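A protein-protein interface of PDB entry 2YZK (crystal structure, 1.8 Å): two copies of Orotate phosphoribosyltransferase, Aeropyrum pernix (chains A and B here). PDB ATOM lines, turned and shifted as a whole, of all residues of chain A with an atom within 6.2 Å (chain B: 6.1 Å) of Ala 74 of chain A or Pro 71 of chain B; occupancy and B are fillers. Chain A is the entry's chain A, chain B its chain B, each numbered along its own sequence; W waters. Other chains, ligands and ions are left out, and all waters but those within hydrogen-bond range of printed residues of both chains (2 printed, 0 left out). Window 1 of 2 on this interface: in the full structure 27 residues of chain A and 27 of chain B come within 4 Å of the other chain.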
ATOM      1  N   VAL A  62     -15.106  20.601  21.713  1.00  0.00           N
ATOM      2  CA  VAL A  62     -15.773  20.068  20.535  1.00  0.00           C
ATOM      3  C   VAL A  62     -17.257  20.106  20.893  1.00  0.00           C
ATOM      4  O   VAL A  62     -17.646  19.645  21.963  1.00  0.00           O
ATOM      5  CB  VAL A  62     -15.375  18.605  20.258  1.00  0.00           C
ATOM      6  CG1 VAL A  62     -16.038  18.134  18.975  1.00  0.00           C
ATOM      7  CG2 VAL A  62     -13.860  18.476  20.147  1.00  0.00           C
ATOM      8  N   GLY A  69     -25.015  14.220  15.535  1.00  0.00           N
ATOM      9  CA  GLY A  69     -23.595  14.494  15.644  1.00  0.00           C
ATOM     10  C   GLY A  69     -22.998  14.259  17.019  1.00  0.00           C
ATOM     11  O   GLY A  69     -21.786  14.378  17.193  1.00  0.00           O
ATOM     12  N   LEU A  70     -23.831  13.899  17.990  1.00  0.00           N
ATOM     13  CA  LEU A  70     -23.342  13.704  19.352  1.00  0.00           C
ATOM     14  C   LEU A  70     -22.319  12.582  19.551  1.00  0.00           C
ATOM     15  O   LEU A  70     -21.288  12.799  20.178  1.00  0.00           O
ATOM     16  CB  LEU A  70     -24.523  13.531  20.317  1.00  0.00           C
ATOM     17  CG  LEU A  70     -24.199  13.602  21.813  1.00  0.00           C
ATOM     18  CD1 LEU A  70     -23.295  14.790  22.121  1.00  0.00           C
ATOM     19  CD2 LEU A  70     -25.496  13.691  22.596  1.00  0.00           C
ATOM     20  N   PRO A  71     -22.577  11.374  19.024  1.00  0.00           N
ATOM     21  CA  PRO A  71     -21.576  10.320  19.229  1.00  0.00           C
ATOM     22  C   PRO A  71     -20.237  10.708  18.614  1.00  0.00           C
ATOM     23  O   PRO A  71     -19.174  10.458  19.191  1.00  0.00           O
ATOM     24  CB  PRO A  71     -22.193   9.116  18.530  1.00  0.00           C
ATOM     25  CG  PRO A  71     -23.669   9.364  18.677  1.00  0.00           C
ATOM     26  CD  PRO A  71     -23.776  10.834  18.363  1.00  0.00           C
ATOM     27  N   TRP A  72     -20.296  11.324  17.437  1.00  0.00           N
ATOM     28  CA  TRP A  72     -19.091  11.747  16.744  1.00  0.00           C
ATOM     29  C   TRP A  72     -18.322  12.795  17.536  1.00  0.00           C
ATOM     30  O   TRP A  72     -17.102  12.701  17.674  1.00  0.00           O
ATOM     31  CB  TRP A  72     -19.445  12.288  15.360  1.00  0.00           C
ATOM     32  CG  TRP A  72     -20.128  11.266  14.525  1.00  0.00           C
ATOM     33  CD1 TRP A  72     -21.450  11.230  14.197  1.00  0.00           C
ATOM     34  CD2 TRP A  72     -19.541  10.082  13.971  1.00  0.00           C
ATOM     35  NE1 TRP A  72     -21.729  10.095  13.473  1.00  0.00           N
ATOM     36  CE2 TRP A  72     -20.575   9.371  13.322  1.00  0.00           C
ATOM     37  CE3 TRP A  72     -18.244   9.552  13.962  1.00  0.00           C
ATOM     38  CZ2 TRP A  72     -20.355   8.153  12.668  1.00  0.00           C
ATOM     39  CZ3 TRP A  72     -18.021   8.334  13.310  1.00  0.00           C
ATOM     40  CH2 TRP A  72     -19.077   7.652  12.673  1.00  0.00           C
ATOM     41  N   ALA A  73     -19.038  13.786  18.061  1.00  0.00           N
ATOM     42  CA  ALA A  73     -18.412  14.843  18.846  1.00  0.00           C
ATOM     43  C   ALA A  73     -17.787  14.262  20.108  1.00  0.00           C
ATOM     44  O   ALA A  73     -16.667  14.618  20.478  1.00  0.00           O
ATOM     45  CB  ALA A  73     -19.441  15.904  19.220  1.00  0.00           C
ATOM     46  N   ALA A  74     -18.513  13.363  20.767  1.00  0.00           N
ATOM     47  CA  ALA A  74     -18.011  12.748  21.994  1.00  0.00           C
ATOM     48  C   ALA A  74     -16.745  11.937  21.730  1.00  0.00           C
ATOM     49  O   ALA A  74     -15.793  12.000  22.503  1.00  0.00           O
ATOM     50  CB  ALA A  74     -19.088  11.856  22.619  1.00  0.00           C
ATOM     51  N   MET A  75     -16.738  11.175  20.640  1.00  0.00           N
ATOM     52  CA  MET A  75     -15.577  10.364  20.305  1.00  0.00           C
ATOM     53  C   MET A  75     -14.380  11.232  19.927  1.00  0.00           C
ATOM     54  O   MET A  75     -13.252  10.904  20.272  1.00  0.00           O
ATOM     55  CB  MET A  75     -15.932   9.379  19.187  1.00  0.00           C
ATOM     56  CG  MET A  75     -17.023   8.397  19.609  1.00  0.00           C
ATOM     57  SD  MET A  75     -17.621   7.335  18.276  1.00  0.00           S
ATOM     58  CE  MET A  75     -16.233   6.203  18.194  1.00  0.00           C
ATOM     59  N   LEU A  76     -14.629  12.332  19.222  1.00  0.00           N
ATOM     60  CA  LEU A  76     -13.556  13.252  18.846  1.00  0.00           C
ATOM     61  C   LEU A  76     -12.980  13.932  20.084  1.00  0.00           C
ATOM     62  O   LEU A  76     -11.765  14.105  20.203  1.00  0.00           O
ATOM     63  CB  LEU A  76     -14.069  14.321  17.880  1.00  0.00           C
ATOM     64  CG  LEU A  76     -14.385  13.860  16.459  1.00  0.00           C
ATOM     65  CD1 LEU A  76     -15.090  14.986  15.706  1.00  0.00           C
ATOM     66  CD2 LEU A  76     -13.090  13.448  15.748  1.00  0.00           C
ATOM     67  N   ALA A  77     -13.854  14.325  21.003  1.00  0.00           N
ATOM     68  CA  ALA A  77     -13.413  14.979  22.228  1.00  0.00           C
ATOM     69  C   ALA A  77     -12.520  14.044  23.042  1.00  0.00           C
ATOM     70  O   ALA A  77     -11.495  14.469  23.575  1.00  0.00           O
ATOM     71  CB  ALA A  77     -14.625  15.425  23.055  1.00  0.00           C
ATOM     72  N   LEU A  78     -12.897  12.771  23.132  1.00  0.00           N
ATOM     73  CA  LEU A  78     -12.092  11.805  23.877  1.00  0.00           C
ATOM     74  C   LEU A  78     -10.736  11.589  23.197  1.00  0.00           C
ATOM     75  O   LEU A  78      -9.697  11.531  23.862  1.00  0.00           O
ATOM     76  CB  LEU A  78     -12.834  10.464  23.997  1.00  0.00           C
ATOM     77  CG  LEU A  78     -12.148   9.358  24.818  1.00  0.00           C
ATOM     78  CD1 LEU A  78     -11.888   9.843  26.241  1.00  0.00           C
ATOM     79  CD2 LEU A  78     -13.022   8.114  24.833  1.00  0.00           C
ATOM     80  N   ARG A  79     -10.746  11.472  21.871  1.00  0.00           N
ATOM     81  CA  ARG A  79      -9.507  11.266  21.123  1.00  0.00           C
ATOM     82  C   ARG A  79      -8.560  12.444  21.321  1.00  0.00           C
ATOM     83  O   ARG A  79      -7.344  12.272  21.393  1.00  0.00           O
ATOM     84  CB  ARG A  79      -9.797  11.097  19.623  1.00  0.00           C
ATOM     85  CG  ARG A  79     -10.426   9.759  19.222  1.00  0.00           C
ATOM     86  CD  ARG A  79      -9.420   8.614  19.308  1.00  0.00           C
ATOM     87  NE  ARG A  79      -8.321   8.788  18.362  1.00  0.00           N
ATOM     88  CZ  ARG A  79      -8.419   8.599  17.050  1.00  0.00           C
ATOM     89  NH1 ARG A  79      -9.569   8.220  16.512  1.00  0.00           N
ATOM     90  NH2 ARG A  79      -7.368   8.811  16.267  1.00  0.00           N
ATOM     91  N   LEU A  84     -16.194  18.472  26.043  1.00  0.00           N
ATOM     92  CA  LEU A  84     -17.285  18.222  25.118  1.00  0.00           C
ATOM     93  C   LEU A  84     -18.494  19.044  25.533  1.00  0.00           C
ATOM     94  O   LEU A  84     -18.713  19.311  26.713  1.00  0.00           O
ATOM     95  CB  LEU A  84     -17.677  16.735  25.113  1.00  0.00           C
ATOM     96  CG  LEU A  84     -18.981  16.411  24.372  1.00  0.00           C
ATOM     97  CD1 LEU A  84     -18.783  16.586  22.858  1.00  0.00           C
ATOM     98  CD2 LEU A  84     -19.415  14.979  24.695  1.00  0.00           C
ATOM     99  N   TYR A  86     -22.691  20.149  23.794  1.00  0.00           N
ATOM    100  CA  TYR A  86     -23.628  19.862  22.718  1.00  0.00           C
ATOM    101  C   TYR A  86     -24.905  20.647  22.860  1.00  0.00           C
ATOM    102  O   TYR A  86     -25.276  21.086  23.956  1.00  0.00           O
ATOM    103  CB  TYR A  86     -23.920  18.355  22.611  1.00  0.00           C
ATOM    104  CG  TYR A  86     -24.601  17.705  23.797  1.00  0.00           C
ATOM    105  CD1 TYR A  86     -25.991  17.622  23.870  1.00  0.00           C
ATOM    106  CD2 TYR A  86     -23.851  17.094  24.804  1.00  0.00           C
ATOM    107  CE1 TYR A  86     -26.617  16.934  24.911  1.00  0.00           C
ATOM    108  CE2 TYR A  86     -24.466  16.408  25.848  1.00  0.00           C
ATOM    109  CZ  TYR A  86     -25.849  16.328  25.893  1.00  0.00           C
ATOM    110  OH  TYR A  86     -26.459  15.619  26.902  1.00  0.00           O
ATOM    111  N   LEU B  35     -19.013  16.375  31.233  1.00  0.00           N
ATOM    112  CA  LEU B  35     -18.501  16.300  29.869  1.00  0.00           C
ATOM    113  C   LEU B  35     -17.688  17.516  29.440  1.00  0.00           C
ATOM    114  O   LEU B  35     -16.853  17.416  28.546  1.00  0.00           O
ATOM    115  CB  LEU B  35     -19.663  16.070  28.888  1.00  0.00           C
ATOM    116  CG  LEU B  35     -20.425  14.759  29.125  1.00  0.00           C
ATOM    117  CD1 LEU B  35     -21.711  14.759  28.307  1.00  0.00           C
ATOM    118  CD2 LEU B  35     -19.540  13.558  28.763  1.00  0.00           C
ATOM    119  N   TYR B  41     -14.530  13.983  33.073  1.00  0.00           N
ATOM    120  CA  TYR B  41     -15.126  12.840  32.388  1.00  0.00           C
ATOM    121  C   TYR B  41     -14.186  11.652  32.273  1.00  0.00           C
ATOM    122  O   TYR B  41     -14.643  10.520  32.152  1.00  0.00           O
ATOM    123  CB  TYR B  41     -15.700  13.231  31.007  1.00  0.00           C
ATOM    124  CG  TYR B  41     -14.724  13.567  29.893  1.00  0.00           C
ATOM    125  CD1 TYR B  41     -13.837  12.614  29.394  1.00  0.00           C
ATOM    126  CD2 TYR B  41     -14.766  14.814  29.263  1.00  0.00           C
ATOM    127  CE1 TYR B  41     -13.025  12.889  28.292  1.00  0.00           C
ATOM    128  CE2 TYR B  41     -13.959  15.098  28.161  1.00  0.00           C
ATOM    129  CZ  TYR B  41     -13.093  14.130  27.677  1.00  0.00           C
ATOM    130  OH  TYR B  41     -12.321  14.386  26.566  1.00  0.00           O
ATOM    131  N   LEU B  45     -15.284   8.009  33.299  1.00  0.00           N
ATOM    132  CA  LEU B  45     -15.149   6.873  32.392  1.00  0.00           C
ATOM    133  C   LEU B  45     -14.349   5.768  33.065  1.00  0.00           C
ATOM    134  O   LEU B  45     -14.675   4.593  32.927  1.00  0.00           O
ATOM    135  CB  LEU B  45     -14.443   7.280  31.092  1.00  0.00           C
ATOM    136  CG  LEU B  45     -15.228   8.148  30.105  1.00  0.00           C
ATOM    137  CD1 LEU B  45     -14.299   8.566  28.972  1.00  0.00           C
ATOM    138  CD2 LEU B  45     -16.434   7.380  29.557  1.00  0.00           C
ATOM    139  N   THR B  67     -30.534  11.002  25.211  1.00  0.00           N
ATOM    140  CA  THR B  67     -29.316  11.635  24.704  1.00  0.00           C
ATOM    141  C   THR B  67     -28.202  11.748  25.739  1.00  0.00           C
ATOM    142  O   THR B  67     -27.034  11.778  25.378  1.00  0.00           O
ATOM    143  CB  THR B  67     -29.586  13.031  24.093  1.00  0.00           C
ATOM    144  OG1 THR B  67     -29.803  13.984  25.135  1.00  0.00           O
ATOM    145  CG2 THR B  67     -30.808  12.981  23.185  1.00  0.00           C
ATOM    146  N   GLY B  68     -28.910  11.683  26.889  1.00  0.00           N
ATOM    147  CA  GLY B  68     -28.160  11.712  28.137  1.00  0.00           C
ATOM    148  C   GLY B  68     -27.027  10.713  28.293  1.00  0.00           C
ATOM    149  O   GLY B  68     -25.897  11.079  28.636  1.00  0.00           O
ATOM    150  N   GLY B  69     -27.317   9.443  28.049  1.00  0.00           N
ATOM    151  CA  GLY B  69     -26.288   8.428  28.178  1.00  0.00           C
ATOM    152  C   GLY B  69     -25.515   8.203  26.894  1.00  0.00           C
ATOM    153  O   GLY B  69     -24.642   7.336  26.834  1.00  0.00           O
ATOM    154  N   LEU B  70     -25.807   8.996  25.870  1.00  0.00           N
ATOM    155  CA  LEU B  70     -25.141   8.800  24.599  1.00  0.00           C
ATOM    156  C   LEU B  70     -23.658   9.142  24.580  1.00  0.00           C
ATOM    157  O   LEU B  70     -22.860   8.362  24.066  1.00  0.00           O
ATOM    158  CB  LEU B  70     -25.887   9.542  23.483  1.00  0.00           C
ATOM    159  CG  LEU B  70     -25.458   9.181  22.049  1.00  0.00           C
ATOM    160  CD1 LEU B  70     -25.333   7.669  21.879  1.00  0.00           C
ATOM    161  CD2 LEU B  70     -26.477   9.744  21.071  1.00  0.00           C
ATOM    162  N   PRO B  71     -23.259  10.303  25.131  1.00  0.00           N
ATOM    163  CA  PRO B  71     -21.825  10.611  25.104  1.00  0.00           C
ATOM    164  C   PRO B  71     -21.009   9.575  25.884  1.00  0.00           C
ATOM    165  O   PRO B  71     -19.923   9.168  25.460  1.00  0.00           O
ATOM    166  CB  PRO B  71     -21.756  11.990  25.749  1.00  0.00           C
ATOM    167  CG  PRO B  71     -23.079  12.602  25.379  1.00  0.00           C
ATOM    168  CD  PRO B  71     -24.033  11.457  25.621  1.00  0.00           C
ATOM    169  N   TRP B  72     -21.536   9.155  27.032  1.00  0.00           N
ATOM    170  CA  TRP B  72     -20.842   8.179  27.867  1.00  0.00           C
ATOM    171  C   TRP B  72     -20.704   6.839  27.142  1.00  0.00           C
ATOM    172  O   TRP B  72     -19.630   6.228  27.138  1.00  0.00           O
ATOM    173  CB  TRP B  72     -21.586   7.997  29.193  1.00  0.00           C
ATOM    174  CG  TRP B  72     -21.700   9.274  29.972  1.00  0.00           C
ATOM    175  CD1 TRP B  72     -22.818  10.040  30.142  1.00  0.00           C
ATOM    176  CD2 TRP B  72     -20.637   9.960  30.639  1.00  0.00           C
ATOM    177  NE1 TRP B  72     -22.513  11.166  30.869  1.00  0.00           N
ATOM    178  CE2 TRP B  72     -21.182  11.143  31.187  1.00  0.00           C
ATOM    179  CE3 TRP B  72     -19.272   9.693  30.824  1.00  0.00           C
ATOM    180  CZ2 TRP B  72     -20.411  12.056  31.908  1.00  0.00           C
ATOM    181  CZ3 TRP B  72     -18.504  10.601  31.540  1.00  0.00           C
ATOM    182  CH2 TRP B  72     -19.078  11.772  32.074  1.00  0.00           C
ATOM    183  N   ALA B  73     -21.788   6.383  26.523  1.00  0.00           N
ATOM    184  CA  ALA B  73     -21.750   5.123  25.793  1.00  0.00           C
ATOM    185  C   ALA B  73     -20.775   5.205  24.623  1.00  0.00           C
ATOM    186  O   ALA B  73     -20.027   4.263  24.360  1.00  0.00           O
ATOM    187  CB  ALA B  73     -23.145   4.775  25.284  1.00  0.00           C
ATOM    188  N   ALA B  74     -20.781   6.336  23.921  1.00  0.00           N
ATOM    189  CA  ALA B  74     -19.892   6.525  22.778  1.00  0.00           C
ATOM    190  C   ALA B  74     -18.427   6.507  23.205  1.00  0.00           C
ATOM    191  O   ALA B  74     -17.583   5.906  22.537  1.00  0.00           O
ATOM    192  CB  ALA B  74     -20.220   7.847  22.068  1.00  0.00           C
ATOM    193  N   MET B  75     -18.132   7.171  24.318  1.00  0.00           N
ATOM    194  CA  MET B  75     -16.773   7.224  24.830  1.00  0.00           C
ATOM    195  C   MET B  75     -16.339   5.851  25.347  1.00  0.00           C
ATOM    196  O   MET B  75     -15.187   5.467  25.176  1.00  0.00           O
ATOM    197  CB  MET B  75     -16.685   8.289  25.925  1.00  0.00           C
ATOM    198  CG  MET B  75     -16.986   9.678  25.382  1.00  0.00           C
ATOM    199  SD  MET B  75     -17.125  10.957  26.656  1.00  0.00           S
ATOM    200  CE  MET B  75     -15.393  11.085  27.114  1.00  0.00           C
ATOM    201  N   LEU B  76     -17.254   5.112  25.968  1.00  0.00           N
ATOM    202  CA  LEU B  76     -16.911   3.779  26.460  1.00  0.00           C
ATOM    203  C   LEU B  76     -16.654   2.854  25.272  1.00  0.00           C
ATOM    204  O   LEU B  76     -15.702   2.071  25.280  1.00  0.00           O
ATOM    205  CB  LEU B  76     -18.040   3.209  27.330  1.00  0.00           C
ATOM    206  CG  LEU B  76     -18.227   3.808  28.730  1.00  0.00           C
ATOM    207  CD1 LEU B  76     -19.458   3.198  29.388  1.00  0.00           C
ATOM    208  CD2 LEU B  76     -16.980   3.535  29.582  1.00  0.00           C
ATOM    209  N   LEU B  78     -15.561   3.612  22.329  1.00  0.00           N
ATOM    210  CA  LEU B  78     -14.272   3.948  21.749  1.00  0.00           C
ATOM    211  C   LEU B  78     -13.126   3.406  22.594  1.00  0.00           C
ATOM    212  O   LEU B  78     -12.183   2.815  22.063  1.00  0.00           O
ATOM    213  CB  LEU B  78     -14.128   5.464  21.615  1.00  0.00           C
ATOM    214  CG  LEU B  78     -12.855   5.938  20.914  1.00  0.00           C
ATOM    215  CD1 LEU B  78     -12.866   5.439  19.478  1.00  0.00           C
ATOM    216  CD2 LEU B  78     -12.776   7.463  20.950  1.00  0.00           C
HETATM  217  O   HOH W   1     -28.998  15.358  27.002  1.00  0.00           O
HETATM  218  O   HOH W   2     -25.153  13.465  28.236  1.00  0.00           O
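N of Leu 84 of chain A sits at hydrogen-bond distance from O of Leu 35 of chain B (2.8 Å).
O of Ala 77 of chain A sits at hydrogen-bond distance from OH of Tyr 41 of chain B (3.1 Å).
Leu 70 of chain A touches Thr 67 of chain B (CD2 to O, 3.7 Å).
CG of Pro 71 of chain B touches CD2 of Leu 70 of chain A, 3.8 Å away.
Leu 70 of chain B touches Pro 71 of chain A.
Ala 74 of chain A touches Pro 71 of chain B (CB to CA, 3.9 Å).
Met 75 of chain A touches Ala 74 of chain B (CG to O, 3.9 Å).
Leu 78 of chain B touches Met 75 of chain A (CD2 to O, 3.5 Å).
Leu 78 of chain A touches Tyr 41 of chain B.
Leu 78 of chain B touches Leu 78 of chain A.
Arg 79 of chain A touches Leu 78 of chain B.
Pro 71 of chain B touches Leu 84 of chain A (CB to CD2, 3.9 Å).
Trp 72 of chain A touches none of the printed residues of chain B.
Ala 74 of chain A touches just these residues of chain B: Pro 71 (3.9 Å) and Met 75 (3.9 Å).
Of the printed residues of chain B, Ala 77 of chain A touches Tyr 41.
Of the printed residues of chain A, Leu 35 of chain B touches Leu 84.
Pro 71 of chain B touches just these residues of chain A: Leu 70 (3.8 Å), Ala 74 (3.9 Å) and Leu 84 (3.9 Å).
Ala 73 of chain B touches none of the printed residues of chain A.
Of the printed residues of chain A, Leu 78 of chain B touches Met 75, Leu 78 and Arg 79.
The nearest residue of chain B that does not touch Ala 74 of chain A is Ala 74 of chain B (4.2 Å).
The nearest residue of chain A that does not touch Pro 71 of chain B is Tyr 86 of chain A (4.1 Å).
Printed residues of chain B that touch a printed residue of chain A: Leu 35, Tyr 41, Leu 45, Thr 67, Leu 70, Pro 71, Ala 74, Met 75 and Leu 78.
Hydrophobic or aromatic side chains of chain B that line the printed part of chain A: Tyr 41, Leu 45, Leu 70, Pro 71, Met 75 and Leu 78.
Of the 14 printed residues of chain A, 8 touch a printed residue of chain B.
Printed residues of chain A that touch a printed residue of chain B: Leu 70, Pro 71, Ala 74, Met 75, Ala 77, Leu 78, Arg 79 and Leu 84.
Hydrophobic or aromatic side chains of chain A that line the printed part of chain B: Leu 70, Pro 71, Ala 74, Met 75, Leu 78 and Leu 84.
Among the printed residues, no Asp or Glu carboxylate lies within 4 Å of a Lys or Arg side-chain nitrogen of the other chain.
Leu 70 of chain A touches Pro 71 of chain B, and with the chains exchanged Pro 71 of chain A touches Leu 70 of chain B.
Ala 74 of chain A touches Pro 71 of chain B, but with the chains exchanged Pro 71 of chain A does not touch Ala 74 of chain B (4.002 Å).
Met 75 of chain A touches Leu 78 of chain B, and with the chains exchanged Leu 78 of chain A touches Met 75 of chain B.
Leu 78 of chain B touches its own counterpart, Leu 78 of chain A.
Of the 15 pairs that touch across the chains among the printed residues, 7 have their exchanged pair printed and touching as well.
Water W1 lies within hydrogen-bond range of OG1 of Thr 67 of chain B (2.5 Å) and OH of Tyr 86 of chain A (2.6 Å).
Water W2 lies within hydrogen-bond range of O of Gly 68 of chain B (2.5 Å) and OH of Tyr 86 of chain A (2.9 Å).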
